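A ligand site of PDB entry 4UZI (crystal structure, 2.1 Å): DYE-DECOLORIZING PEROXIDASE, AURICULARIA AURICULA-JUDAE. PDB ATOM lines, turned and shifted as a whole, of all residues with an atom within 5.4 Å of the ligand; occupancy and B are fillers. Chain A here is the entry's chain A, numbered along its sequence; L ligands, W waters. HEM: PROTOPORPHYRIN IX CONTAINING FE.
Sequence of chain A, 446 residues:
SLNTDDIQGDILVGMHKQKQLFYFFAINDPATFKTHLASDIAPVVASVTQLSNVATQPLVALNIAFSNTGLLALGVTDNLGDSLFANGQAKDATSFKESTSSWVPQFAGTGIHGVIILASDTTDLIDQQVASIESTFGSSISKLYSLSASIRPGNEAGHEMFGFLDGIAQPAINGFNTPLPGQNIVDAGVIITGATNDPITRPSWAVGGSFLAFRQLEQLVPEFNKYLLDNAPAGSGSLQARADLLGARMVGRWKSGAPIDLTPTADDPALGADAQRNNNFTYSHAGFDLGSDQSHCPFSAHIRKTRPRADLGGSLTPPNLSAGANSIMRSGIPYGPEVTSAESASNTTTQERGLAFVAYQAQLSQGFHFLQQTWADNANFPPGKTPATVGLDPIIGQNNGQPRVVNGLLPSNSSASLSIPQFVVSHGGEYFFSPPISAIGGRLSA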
ATOM      1  N   GLU A 160     -21.371  19.841  14.764  1.00  0.00           N
ATOM      2  CA  GLU A 160     -20.719  18.740  15.471  1.00  0.00           C
ATOM      3  C   GLU A 160     -19.222  18.769  15.197  1.00  0.00           C
ATOM      4  O   GLU A 160     -18.723  19.650  14.481  1.00  0.00           O
ATOM      5  CB  GLU A 160     -21.332  17.401  15.095  1.00  0.00           C
ATOM      6  CG  GLU A 160     -21.400  17.124  13.592  1.00  0.00           C
ATOM      7  CD  GLU A 160     -20.027  16.914  12.987  1.00  0.00           C
ATOM      8  OE1 GLU A 160     -19.338  15.950  13.389  1.00  0.00           O
ATOM      9  OE2 GLU A 160     -19.617  17.725  12.130  1.00  0.00           O
ATOM     10  N   PHE A 162     -16.970  17.133  13.587  1.00  0.00           N
ATOM     11  CA  PHE A 162     -16.420  17.051  12.231  1.00  0.00           C
ATOM     12  C   PHE A 162     -16.600  18.381  11.500  1.00  0.00           C
ATOM     13  O   PHE A 162     -16.015  18.591  10.435  1.00  0.00           O
ATOM     14  CB  PHE A 162     -17.060  15.909  11.431  1.00  0.00           C
ATOM     15  CG  PHE A 162     -16.571  14.536  11.813  1.00  0.00           C
ATOM     16  CD1 PHE A 162     -15.253  14.327  12.168  1.00  0.00           C
ATOM     17  CD2 PHE A 162     -17.438  13.459  11.792  1.00  0.00           C
ATOM     18  CE1 PHE A 162     -14.803  13.068  12.530  1.00  0.00           C
ATOM     19  CE2 PHE A 162     -16.998  12.182  12.144  1.00  0.00           C
ATOM     20  CZ  PHE A 162     -15.679  11.998  12.517  1.00  0.00           C
ATOM     21  N   PHE A 164     -19.834  19.862  10.802  1.00  0.00           N
ATOM     22  CA  PHE A 164     -21.082  19.951  10.033  1.00  0.00           C
ATOM     23  C   PHE A 164     -22.204  20.495  10.890  1.00  0.00           C
ATOM     24  O   PHE A 164     -22.362  20.090  12.051  1.00  0.00           O
ATOM     25  CB  PHE A 164     -21.463  18.584   9.456  1.00  0.00           C
ATOM     26  CG  PHE A 164     -20.503  18.071   8.435  1.00  0.00           C
ATOM     27  CD1 PHE A 164     -19.294  17.511   8.820  1.00  0.00           C
ATOM     28  CD2 PHE A 164     -20.776  18.173   7.079  1.00  0.00           C
ATOM     29  CE1 PHE A 164     -18.375  17.076   7.885  1.00  0.00           C
ATOM     30  CE2 PHE A 164     -19.863  17.729   6.144  1.00  0.00           C
ATOM     31  CZ  PHE A 164     -18.654  17.193   6.547  1.00  0.00           C
ATOM     32  N   LEU A 165     -22.985  21.416  10.334  1.00  0.00           N
ATOM     33  CA  LEU A 165     -24.178  21.903  11.012  1.00  0.00           C
ATOM     34  C   LEU A 165     -25.143  20.770  11.318  1.00  0.00           C
ATOM     35  O   LEU A 165     -25.438  19.946  10.450  1.00  0.00           O
ATOM     36  CB  LEU A 165     -24.882  22.993  10.185  1.00  0.00           C
ATOM     37  CG  LEU A 165     -26.038  23.674  10.918  1.00  0.00           C
ATOM     38  CD1 LEU A 165     -25.545  24.487  12.108  1.00  0.00           C
ATOM     39  CD2 LEU A 165     -26.859  24.542   9.974  1.00  0.00           C
ATOM     40  N   ASP A 166     -25.627  20.744  12.554  1.00  0.00           N
ATOM     41  CA  ASP A 166     -26.428  19.638  13.079  1.00  0.00           C
ATOM     42  C   ASP A 166     -27.809  20.139  13.497  1.00  0.00           C
ATOM     43  O   ASP A 166     -28.044  21.350  13.586  1.00  0.00           O
ATOM     44  CB  ASP A 166     -25.724  19.021  14.302  1.00  0.00           C
ATOM     45  CG  ASP A 166     -26.261  17.644  14.659  1.00  0.00           C
ATOM     46  OD1 ASP A 166     -27.031  17.060  13.865  1.00  0.00           O
ATOM     47  OD2 ASP A 166     -25.887  17.130  15.741  1.00  0.00           O
ATOM     48  N   GLY A 167     -28.721  19.201  13.750  1.00  0.00           N
ATOM     49  CA  GLY A 167     -30.050  19.529  14.268  1.00  0.00           C
ATOM     50  C   GLY A 167     -30.992  20.153  13.258  1.00  0.00           C
ATOM     51  O   GLY A 167     -32.002  20.746  13.618  1.00  0.00           O
ATOM     52  N   ILE A 168     -30.676  19.980  11.974  1.00  0.00           N
ATOM     53  CA  ILE A 168     -31.523  20.524  10.908  1.00  0.00           C
ATOM     54  C   ILE A 168     -32.777  19.676  10.733  1.00  0.00           C
ATOM     55  O   ILE A 168     -33.877  20.205  10.575  1.00  0.00           O
ATOM     56  CB  ILE A 168     -30.750  20.603   9.574  1.00  0.00           C
ATOM     57  CG1 ILE A 168     -29.593  21.607   9.683  1.00  0.00           C
ATOM     58  CG2 ILE A 168     -31.679  21.010   8.447  1.00  0.00           C
ATOM     59  CD1 ILE A 168     -28.432  21.306   8.765  1.00  0.00           C
ATOM     60  N   ALA A 169     -32.602  18.359  10.830  1.00  0.00           N
ATOM     61  CA  ALA A 169     -33.635  17.418  10.408  1.00  0.00           C
ATOM     62  C   ALA A 169     -34.195  16.660  11.610  1.00  0.00           C
ATOM     63  O   ALA A 169     -33.452  15.986  12.326  1.00  0.00           O
ATOM     64  CB  ALA A 169     -33.058  16.429   9.404  1.00  0.00           C
ATOM     65  N   GLN A 170     -35.495  16.799  11.828  1.00  0.00           N
ATOM     66  CA  GLN A 170     -36.191  16.030  12.844  1.00  0.00           C
ATOM     67  C   GLN A 170     -37.553  15.632  12.284  1.00  0.00           C
ATOM     68  O   GLN A 170     -38.108  16.334  11.455  1.00  0.00           O
ATOM     69  CB  GLN A 170     -36.383  16.863  14.117  1.00  0.00           C
ATOM     70  CG  GLN A 170     -35.139  17.604  14.577  1.00  0.00           C
ATOM     71  CD  GLN A 170     -34.392  16.861  15.669  1.00  0.00           C
ATOM     72  OE1 GLN A 170     -34.481  15.633  15.770  1.00  0.00           O
ATOM     73  NE2 GLN A 170     -33.653  17.601  16.481  1.00  0.00           N
ATOM     74  N   LEU A 217     -19.955   8.758  21.530  1.00  0.00           N
ATOM     75  CA  LEU A 217     -19.293   8.412  20.275  1.00  0.00           C
ATOM     76  C   LEU A 217     -18.084   9.297  20.039  1.00  0.00           C
ATOM     77  O   LEU A 217     -18.229  10.509  19.776  1.00  0.00           O
ATOM     78  CB  LEU A 217     -20.279   8.503  19.123  1.00  0.00           C
ATOM     79  CG  LEU A 217     -21.574   7.693  19.264  1.00  0.00           C
ATOM     80  CD1 LEU A 217     -22.573   8.014  18.165  1.00  0.00           C
ATOM     81  CD2 LEU A 217     -21.263   6.205  19.280  1.00  0.00           C
ATOM     82  N   GLN A 219     -15.104  11.014  18.150  1.00  0.00           N
ATOM     83  CA  GLN A 219     -14.821  11.358  16.772  1.00  0.00           C
ATOM     84  C   GLN A 219     -13.338  11.617  16.562  1.00  0.00           C
ATOM     85  O   GLN A 219     -12.701  12.295  17.353  1.00  0.00           O
ATOM     86  CB  GLN A 219     -15.641  12.574  16.360  1.00  0.00           C
ATOM     87  CG  GLN A 219     -17.133  12.276  16.297  1.00  0.00           C
ATOM     88  CD  GLN A 219     -17.949  13.513  16.027  1.00  0.00           C
ATOM     89  OE1 GLN A 219     -18.646  14.012  16.912  1.00  0.00           O
ATOM     90  NE2 GLN A 219     -17.848  14.046  14.811  1.00  0.00           N
ATOM     91  N   VAL A 251     -21.520  12.742   4.330  1.00  0.00           N
ATOM     92  CA  VAL A 251     -22.563  13.143   5.267  1.00  0.00           C
ATOM     93  C   VAL A 251     -23.913  13.243   4.582  1.00  0.00           C
ATOM     94  O   VAL A 251     -24.940  12.814   5.135  1.00  0.00           O
ATOM     95  CB  VAL A 251     -22.210  14.480   5.966  1.00  0.00           C
ATOM     96  CG1 VAL A 251     -23.275  14.859   6.973  1.00  0.00           C
ATOM     97  CG2 VAL A 251     -20.858  14.366   6.653  1.00  0.00           C
ATOM     98  N   ARG A 253     -24.681  16.298   3.565  1.00  0.00           N
ATOM     99  CA  ARG A 253     -24.782  17.757   3.630  1.00  0.00           C
ATOM    100  C   ARG A 253     -23.389  18.361   3.559  1.00  0.00           C
ATOM    101  O   ARG A 253     -22.421  17.714   3.954  1.00  0.00           O
ATOM    102  CB  ARG A 253     -25.469  18.207   4.930  1.00  0.00           C
ATOM    103  CG  ARG A 253     -26.977  17.955   4.961  1.00  0.00           C
ATOM    104  CD  ARG A 253     -27.608  18.476   6.243  1.00  0.00           C
ATOM    105  NE  ARG A 253     -28.970  17.960   6.390  1.00  0.00           N
ATOM    106  CZ  ARG A 253     -30.033  18.504   5.828  1.00  0.00           C
ATOM    107  NH1 ARG A 253     -29.912  19.630   5.120  1.00  0.00           N
ATOM    108  NH2 ARG A 253     -31.224  17.940   5.959  1.00  0.00           N
ATOM    109  N   ASN A 279     -34.288  21.233   3.822  1.00  0.00           N
ATOM    110  CA  ASN A 279     -34.752  19.855   3.987  1.00  0.00           C
ATOM    111  C   ASN A 279     -35.716  19.451   2.884  1.00  0.00           C
ATOM    112  O   ASN A 279     -36.324  18.373   2.929  1.00  0.00           O
ATOM    113  CB  ASN A 279     -35.417  19.637   5.346  1.00  0.00           C
ATOM    114  CG  ASN A 279     -35.082  18.284   5.943  1.00  0.00           C
ATOM    115  OD1 ASN A 279     -34.115  17.649   5.539  1.00  0.00           O
ATOM    116  ND2 ASN A 279     -35.873  17.842   6.917  1.00  0.00           N
ATOM    117  N   TYR A 283     -34.475  12.945  -2.647  1.00  0.00           N
ATOM    118  CA  TYR A 283     -33.456  12.154  -3.351  1.00  0.00           C
ATOM    119  C   TYR A 283     -33.824  11.845  -4.800  1.00  0.00           C
ATOM    120  O   TYR A 283     -32.959  11.458  -5.586  1.00  0.00           O
ATOM    121  CB  TYR A 283     -33.084  10.871  -2.601  1.00  0.00           C
ATOM    122  CG  TYR A 283     -32.446  11.148  -1.265  1.00  0.00           C
ATOM    123  CD1 TYR A 283     -31.289  11.919  -1.170  1.00  0.00           C
ATOM    124  CD2 TYR A 283     -33.027  10.701  -0.091  1.00  0.00           C
ATOM    125  CE1 TYR A 283     -30.729  12.204   0.049  1.00  0.00           C
ATOM    126  CE2 TYR A 283     -32.481  10.984   1.127  1.00  0.00           C
ATOM    127  CZ  TYR A 283     -31.340  11.742   1.200  1.00  0.00           C
ATOM    128  OH  TYR A 283     -30.802  12.018   2.427  1.00  0.00           O
ATOM    129  N   HIS A 302     -24.532   9.390   5.099  1.00  0.00           N
ATOM    130  CA  HIS A 302     -25.116   9.262   6.442  1.00  0.00           C
ATOM    131  C   HIS A 302     -26.615   9.557   6.495  1.00  0.00           C
ATOM    132  O   HIS A 302     -27.392   8.706   6.904  1.00  0.00           O
ATOM    133  CB  HIS A 302     -24.384  10.177   7.427  1.00  0.00           C
ATOM    134  CG  HIS A 302     -24.930  10.120   8.819  1.00  0.00           C
ATOM    135  ND1 HIS A 302     -25.045   8.951   9.532  1.00  0.00           N
ATOM    136  CD2 HIS A 302     -25.323  11.115   9.660  1.00  0.00           C
ATOM    137  CE1 HIS A 302     -25.511   9.220  10.738  1.00  0.00           C
ATOM    138  NE2 HIS A 302     -25.691  10.527  10.836  1.00  0.00           N
ATOM    139  N   ILE A 303     -27.020  10.784   6.164  1.00  0.00           N
ATOM    140  CA  ILE A 303     -28.421  11.167   6.327  1.00  0.00           C
ATOM    141  C   ILE A 303     -29.334  10.343   5.423  1.00  0.00           C
ATOM    142  O   ILE A 303     -30.497  10.101   5.758  1.00  0.00           O
ATOM    143  CB  ILE A 303     -28.650  12.673   6.088  1.00  0.00           C
ATOM    144  CG1 ILE A 303     -28.302  13.069   4.654  1.00  0.00           C
ATOM    145  CG2 ILE A 303     -27.869  13.504   7.091  1.00  0.00           C
ATOM    146  CD1 ILE A 303     -28.809  14.455   4.278  1.00  0.00           C
ATOM    147  N   THR A 306     -29.870   7.130   7.118  1.00  0.00           N
ATOM    148  CA  THR A 306     -30.652   7.230   8.350  1.00  0.00           C
ATOM    149  C   THR A 306     -32.061   7.796   8.174  1.00  0.00           C
ATOM    150  O   THR A 306     -32.944   7.556   8.996  1.00  0.00           O
ATOM    151  CB  THR A 306     -29.916   8.043   9.429  1.00  0.00           C
ATOM    152  OG1 THR A 306     -29.650   9.359   8.929  1.00  0.00           O
ATOM    153  CG2 THR A 306     -28.596   7.355   9.807  1.00  0.00           C
ATOM    154  N   ARG A 307     -32.264   8.593   7.120  1.00  0.00           N
ATOM    155  CA  ARG A 307     -33.619   8.816   6.604  1.00  0.00           C
ATOM    156  C   ARG A 307     -33.679   8.583   5.098  1.00  0.00           C
ATOM    157  O   ARG A 307     -33.389   9.480   4.313  1.00  0.00           O
ATOM    158  CB  ARG A 307     -34.143  10.206   6.949  1.00  0.00           C
ATOM    159  CG  ARG A 307     -35.633  10.376   6.671  1.00  0.00           C
ATOM    160  CD  ARG A 307     -36.083  11.828   6.604  1.00  0.00           C
ATOM    161  NE  ARG A 307     -37.408  11.946   5.972  1.00  0.00           N
ATOM    162  CZ  ARG A 307     -37.940  13.080   5.527  1.00  0.00           C
ATOM    163  NH1 ARG A 307     -37.286  14.234   5.665  1.00  0.00           N
ATOM    164  NH2 ARG A 307     -39.117  13.068   4.936  1.00  0.00           N
ATOM    165  N   ARG A 309     -35.984   8.314   2.929  1.00  0.00           N
ATOM    166  CA  ARG A 309     -36.963   9.047   2.125  1.00  0.00           C
ATOM    167  C   ARG A 309     -37.413   8.204   0.926  1.00  0.00           C
ATOM    168  O   ARG A 309     -37.801   7.054   1.089  1.00  0.00           O
ATOM    169  CB  ARG A 309     -36.392  10.402   1.675  1.00  0.00           C
ATOM    170  CG  ARG A 309     -35.870  11.244   2.836  1.00  0.00           C
ATOM    171  CD  ARG A 309     -35.346  12.608   2.397  1.00  0.00           C
ATOM    172  NE  ARG A 309     -34.626  13.247   3.492  1.00  0.00           N
ATOM    173  CZ  ARG A 309     -34.691  14.543   3.795  1.00  0.00           C
ATOM    174  NH1 ARG A 309     -35.422  15.369   3.065  1.00  0.00           N
ATOM    175  NH2 ARG A 309     -34.043  15.001   4.858  1.00  0.00           N
ATOM    176  N   ILE A 328     -36.363   9.150  14.728  1.00  0.00           N
ATOM    177  CA  ILE A 328     -35.851   9.493  16.055  1.00  0.00           C
ATOM    178  C   ILE A 328     -35.801  11.004  16.211  1.00  0.00           C
ATOM    179  O   ILE A 328     -35.496  11.720  15.255  1.00  0.00           O
ATOM    180  CB  ILE A 328     -34.455   8.887  16.315  1.00  0.00           C
ATOM    181  CG1 ILE A 328     -33.426   9.406  15.313  1.00  0.00           C
ATOM    182  CG2 ILE A 328     -34.511   7.367  16.302  1.00  0.00           C
ATOM    183  CD1 ILE A 328     -31.986   9.074  15.682  1.00  0.00           C
ATOM    184  N   ARG A 330     -33.636  13.873  17.912  1.00  0.00           N
ATOM    185  CA  ARG A 330     -32.208  13.906  18.218  1.00  0.00           C
ATOM    186  C   ARG A 330     -31.863  15.074  19.117  1.00  0.00           C
ATOM    187  O   ARG A 330     -32.177  16.224  18.801  1.00  0.00           O
ATOM    188  CB  ARG A 330     -31.378  13.944  16.939  1.00  0.00           C
ATOM    189  CG  ARG A 330     -31.361  12.615  16.192  1.00  0.00           C
ATOM    190  CD  ARG A 330     -30.628  12.710  14.859  1.00  0.00           C
ATOM    191  NE  ARG A 330     -31.106  13.847  14.066  1.00  0.00           N
ATOM    192  CZ  ARG A 330     -30.336  14.851  13.669  1.00  0.00           C
ATOM    193  NH1 ARG A 330     -29.032  14.838  13.939  1.00  0.00           N
ATOM    194  NH2 ARG A 330     -30.853  15.843  12.968  1.00  0.00           N
ATOM    195  N   LEU A 355     -19.383  13.148  19.995  1.00  0.00           N
ATOM    196  CA  LEU A 355     -20.802  13.484  20.098  1.00  0.00           C
ATOM    197  C   LEU A 355     -21.406  12.745  21.281  1.00  0.00           C
ATOM    198  O   LEU A 355     -21.343  11.520  21.337  1.00  0.00           O
ATOM    199  CB  LEU A 355     -21.534  13.076  18.811  1.00  0.00           C
ATOM    200  CG  LEU A 355     -23.035  13.362  18.753  1.00  0.00           C
ATOM    201  CD1 LEU A 355     -23.320  14.867  18.780  1.00  0.00           C
ATOM    202  CD2 LEU A 355     -23.645  12.706  17.525  1.00  0.00           C
ATOM    203  N   PHE A 357     -24.354  11.399  22.062  1.00  0.00           N
ATOM    204  CA  PHE A 357     -25.501  11.135  21.187  1.00  0.00           C
ATOM    205  C   PHE A 357     -26.715  10.774  22.027  1.00  0.00           C
ATOM    206  O   PHE A 357     -26.655   9.886  22.892  1.00  0.00           O
ATOM    207  CB  PHE A 357     -25.165  10.036  20.174  1.00  0.00           C
ATOM    208  CG  PHE A 357     -26.350   9.527  19.401  1.00  0.00           C
ATOM    209  CD1 PHE A 357     -27.140   8.500  19.909  1.00  0.00           C
ATOM    210  CD2 PHE A 357     -26.615  10.003  18.127  1.00  0.00           C
ATOM    211  CE1 PHE A 357     -28.205   8.003  19.187  1.00  0.00           C
ATOM    212  CE2 PHE A 357     -27.696   9.517  17.401  1.00  0.00           C
ATOM    213  CZ  PHE A 357     -28.486   8.514  17.927  1.00  0.00           C
ATOM    214  N   PHE A 368     -33.263   4.144  17.084  1.00  0.00           N
ATOM    215  CA  PHE A 368     -31.806   4.052  17.021  1.00  0.00           C
ATOM    216  C   PHE A 368     -31.263   2.674  16.637  1.00  0.00           C
ATOM    217  O   PHE A 368     -30.379   2.557  15.793  1.00  0.00           O
ATOM    218  CB  PHE A 368     -31.179   4.472  18.360  1.00  0.00           C
ATOM    219  CG  PHE A 368     -29.812   3.899  18.580  1.00  0.00           C
ATOM    220  CD1 PHE A 368     -28.723   4.372  17.859  1.00  0.00           C
ATOM    221  CD2 PHE A 368     -29.627   2.810  19.429  1.00  0.00           C
ATOM    222  CE1 PHE A 368     -27.472   3.809  18.017  1.00  0.00           C
ATOM    223  CE2 PHE A 368     -28.375   2.247  19.587  1.00  0.00           C
ATOM    224  CZ  PHE A 368     -27.296   2.751  18.891  1.00  0.00           C
ATOM    225  N   LEU A 371     -31.977   1.901  13.014  1.00  0.00           N
ATOM    226  CA  LEU A 371     -31.161   2.706  12.127  1.00  0.00           C
ATOM    227  C   LEU A 371     -29.702   2.242  12.096  1.00  0.00           C
ATOM    228  O   LEU A 371     -29.069   2.246  11.052  1.00  0.00           O
ATOM    229  CB  LEU A 371     -31.242   4.184  12.509  1.00  0.00           C
ATOM    230  CG  LEU A 371     -32.355   4.987  11.837  1.00  0.00           C
ATOM    231  CD1 LEU A 371     -33.695   4.283  12.010  1.00  0.00           C
ATOM    232  CD2 LEU A 371     -32.414   6.398  12.394  1.00  0.00           C
ATOM    233  N   GLN A 372     -29.193   1.816  13.243  1.00  0.00           N
ATOM    234  CA  GLN A 372     -27.781   1.409  13.310  1.00  0.00           C
ATOM    235  C   GLN A 372     -27.551   0.075  12.600  1.00  0.00           C
ATOM    236  O   GLN A 372     -26.653  -0.052  11.770  1.00  0.00           O
ATOM    237  CB  GLN A 372     -27.282   1.355  14.751  1.00  0.00           C
ATOM    238  CG  GLN A 372     -25.794   1.041  14.882  1.00  0.00           C
ATOM    239  CD  GLN A 372     -24.924   2.207  14.453  1.00  0.00           C
ATOM    240  OE1 GLN A 372     -24.976   3.293  15.048  1.00  0.00           O
ATOM    241  NE2 GLN A 372     -24.145   2.008  13.396  1.00  0.00           N
ATOM    242  N   ILE A 395     -20.059   7.425   8.202  1.00  0.00           N
ATOM    243  CA  ILE A 395     -19.980   8.127   9.475  1.00  0.00           C
ATOM    244  C   ILE A 395     -20.083   7.178  10.666  1.00  0.00           C
ATOM    245  O   ILE A 395     -19.226   7.194  11.538  1.00  0.00           O
ATOM    246  CB  ILE A 395     -21.012   9.268   9.586  1.00  0.00           C
ATOM    247  CG1 ILE A 395     -20.860  10.218   8.403  1.00  0.00           C
ATOM    248  CG2 ILE A 395     -20.832  10.007  10.913  1.00  0.00           C
ATOM    249  CD1 ILE A 395     -19.490  10.852   8.265  1.00  0.00           C
ATOM    250  N   ILE A 396     -21.103   6.321  10.676  1.00  0.00           N
ATOM    251  CA  ILE A 396     -21.423   5.527  11.873  1.00  0.00           C
ATOM    252  C   ILE A 396     -21.465   4.024  11.605  1.00  0.00           C
ATOM    253  O   ILE A 396     -21.691   3.241  12.511  1.00  0.00           O
ATOM    254  CB  ILE A 396     -22.776   5.957  12.478  1.00  0.00           C
ATOM    255  CG1 ILE A 396     -23.894   5.784  11.445  1.00  0.00           C
ATOM    256  CG2 ILE A 396     -22.699   7.395  12.964  1.00  0.00           C
ATOM    257  CD1 ILE A 396     -25.290   5.901  12.026  1.00  0.00           C
ATOM    258  N   VAL A 424     -15.611   7.241  13.756  1.00  0.00           N
ATOM    259  CA  VAL A 424     -16.338   7.302  15.011  1.00  0.00           C
ATOM    260  C   VAL A 424     -16.141   6.009  15.782  1.00  0.00           C
ATOM    261  O   VAL A 424     -16.180   4.926  15.202  1.00  0.00           O
ATOM    262  CB  VAL A 424     -17.844   7.519  14.776  1.00  0.00           C
ATOM    263  CG1 VAL A 424     -18.605   7.383  16.098  1.00  0.00           C
ATOM    264  CG2 VAL A 424     -18.090   8.882  14.151  1.00  0.00           C
HETATM  265  CHA HEM L   1     -28.164  13.780  10.705  1.00  0.00           C
HETATM  266  CHB HEM L   1     -23.456  13.587  11.904  1.00  0.00           C
HETATM  267  CHC HEM L   1     -24.352   9.634  14.662  1.00  0.00           C
HETATM  268  CHD HEM L   1     -28.884   9.524  12.904  1.00  0.00           C
HETATM  269  C1A HEM L   1     -26.823  14.050  10.837  1.00  0.00           C
HETATM  270  C2A HEM L   1     -26.202  15.162  10.249  1.00  0.00           C
HETATM  271  C3A HEM L   1     -24.881  15.124  10.575  1.00  0.00           C
HETATM  272  C4A HEM L   1     -24.677  13.974  11.373  1.00  0.00           C
HETATM  273  CMA HEM L   1     -23.835  16.139  10.215  1.00  0.00           C
HETATM  274  CAA HEM L   1     -26.887  16.226   9.418  1.00  0.00           C
HETATM  275  CBA HEM L   1     -27.545  17.262  10.332  1.00  0.00           C
HETATM  276  CGA HEM L   1     -29.052  17.196  10.240  1.00  0.00           C
HETATM  277  O1A HEM L   1     -29.623  16.830   9.181  1.00  0.00           O
HETATM  278  O2A HEM L   1     -29.750  17.535  11.224  1.00  0.00           O
HETATM  279  C1B HEM L   1     -23.311  12.514  12.805  1.00  0.00           C
HETATM  280  C2B HEM L   1     -22.098  12.205  13.490  1.00  0.00           C
HETATM  281  C3B HEM L   1     -22.325  11.092  14.259  1.00  0.00           C
HETATM  282  C4B HEM L   1     -23.746  10.733  14.042  1.00  0.00           C
HETATM  283  CMB HEM L   1     -20.791  12.958  13.337  1.00  0.00           C
HETATM  284  CAB HEM L   1     -21.372  10.365  15.130  1.00  0.00           C
HETATM  285  CBB HEM L   1     -20.702  10.967  16.118  1.00  0.00           C
HETATM  286  C1C HEM L   1     -25.658   9.219  14.379  1.00  0.00           C
HETATM  287  C2C HEM L   1     -26.247   8.000  14.790  1.00  0.00           C
HETATM  288  C3C HEM L   1     -27.533   7.965  14.264  1.00  0.00           C
HETATM  289  C4C HEM L   1     -27.723   9.179  13.543  1.00  0.00           C
HETATM  290  CMC HEM L   1     -25.615   6.924  15.644  1.00  0.00           C
HETATM  291  CAC HEM L   1     -28.542   6.902  14.442  1.00  0.00           C
HETATM  292  CBC HEM L   1     -28.188   5.618  14.423  1.00  0.00           C
HETATM  293  C1D HEM L   1     -28.993  10.741  12.218  1.00  0.00           C
HETATM  294  C2D HEM L   1     -30.293  11.111  11.654  1.00  0.00           C
HETATM  295  C3D HEM L   1     -30.114  12.280  11.034  1.00  0.00           C
HETATM  296  C4D HEM L   1     -28.683  12.620  11.255  1.00  0.00           C
HETATM  297  CMD HEM L   1     -31.586  10.337  11.740  1.00  0.00           C
HETATM  298  CAD HEM L   1     -31.172  13.069  10.302  1.00  0.00           C
HETATM  299  CBD HEM L   1     -31.254  12.593   8.840  1.00  0.00           C
HETATM  300  CGD HEM L   1     -32.523  13.065   8.147  1.00  0.00           C
HETATM  301  O1D HEM L   1     -33.577  13.268   8.809  1.00  0.00           O
HETATM  302  O2D HEM L   1     -32.532  13.222   6.893  1.00  0.00           O
HETATM  303  NA  HEM L   1     -25.866  13.298  11.476  1.00  0.00           N
HETATM  304  NB  HEM L   1     -24.233  11.608  13.134  1.00  0.00           N
HETATM  305  NC  HEM L   1     -26.550   9.878  13.567  1.00  0.00           N
HETATM  306  ND  HEM L   1     -28.047  11.642  11.925  1.00  0.00           N
HETATM  307 FE   HEM L   1     -26.220  11.621  12.490  1.00  0.00          FE
HETATM  308  O   HOH W   1     -35.620  15.020   7.900  1.00  0.00           O
HETATM  309  O   HOH W   2     -30.684  15.611   7.100  1.00  0.00           O
HETATM  310  O   HOH W   3     -34.870  12.787  11.058  1.00  0.00           O
HETATM  311  O   HOH W   4     -32.286  12.155   4.451  1.00  0.00           O
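A ring nitrogen (NE2) of His 302 binds an iron atom (FE) of the ligand (2.1 Å). An oxygen (O2A) of the ligand is in salt-bridge range of the guanidinium group (NH2) of Arg 330 (2.7 Å). N of Ile 168 lies within hydrogen-bond range of O2A of the ligand (2.7 Å). N of Ala 169 sits at hydrogen-bond distance from O2A of the ligand (3.0 Å). The guanidinium group (NE) of Arg 253 is in salt-bridge range of an oxygen (O1A) of the ligand. An oxygen (O2D) of the ligand is in salt-bridge range of the guanidinium group (NH2) of Arg 309 (3.1 Å). O2A of the ligand sits at hydrogen-bond distance from N of Gly 167, at 3.2 Å.
The backbone carbonyl oxygen of His 302 lies within hydrogen-bond range of the side-chain hydroxyl of Thr 306 (3.1 Å). NH1 of Arg 330 lies within salt-bridge range of OD1 of Asp 166 (3.0 Å). The guanidinium group (NH2) of Arg 309 lies within hydrogen-bond range of the side-chain amide oxygen (OD1) of Asn 279 (2.7 Å). The backbone carbonyl oxygen (O) of Ile 396 lies within hydrogen-bond range of the side-chain amide nitrogen (NE2) of Gln 372. N of Phe 164 is in hydrogen-bond range of OE2 of Glu 160 (2.5 Å). The side-chain carboxylate (OE1) of Glu 160 is in hydrogen-bond range of the backbone NH (N) of Phe 162 (2.7 Å). The backbone NH of Leu 355 lies within hydrogen-bond range of the backbone carbonyl oxygen of Leu 217. The backbone carbonyl oxygen of Val 251 is in hydrogen-bond range of the backbone NH of Ile 303 (3.1 Å).
Glu 160 touches the ligand (OE1 to CMB, 3.3 Å). Phe 162 touches the ligand. Phe 164 touches the ligand. O of Leu 165 touches CBA of the ligand, 3.4 Å away. Asp 166 touches the ligand. CB of Leu 217 touches CBB of the ligand, 3.9 Å away. Gln 219 touches the ligand. CG1 of Val 251 touches CMA of the ligand (3.5 Å). Ile 303 touches the ligand. Thr 306 touches the ligand. Arg 307 touches the ligand (CB to O2D, 3.4 Å). Leu 355 touches the ligand. Phe 357 touches the ligand. CD1 of Phe 368 touches CBC of the ligand, at 3.7 Å. Leu 371 touches the ligand. Gln 372 touches the ligand. Ile 395 touches the ligand. Ile 396 touches the ligand (CG2 to CHC, 3.3 Å). CG2 of Val 424 touches CAB of the ligand (3.7 Å). Hydrophobic or aromatic side chains within 4 Å of the ligand: Phe 162, Phe 164, Ile 168, Ala 169, Leu 217, Val 251, His 302, Ile 303, Leu 355, Phe 357, Phe 368, Leu 371, Ile 395, Ile 396 and Val 424. Within 4 Å of the ligand: Glu 160, Phe 162, Phe 164, Leu 165, Asp 166, Gly 167, Ile 168, Ala 169, Leu 217, Gln 219, Val 251, Arg 253, His 302, Ile 303, Thr 306, Arg 307, Arg 309, Arg 330, Leu 355, Phe 357, Phe 368, Leu 371, Gln 372, Ile 395, Ile 396 and Val 424.
Water W2 lies within hydrogen-bond range of an oxygen (O1A) of the ligand and the guanidinium group of Arg 253. Water W4 lies within hydrogen-bond range of the side-chain hydroxyl of Tyr 283, an oxygen (O2D) of the ligand, the guanidinium group of Arg 309, the backbone carbonyl oxygen of Arg 307 and the backbone carbonyl oxygen of Ile 303.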
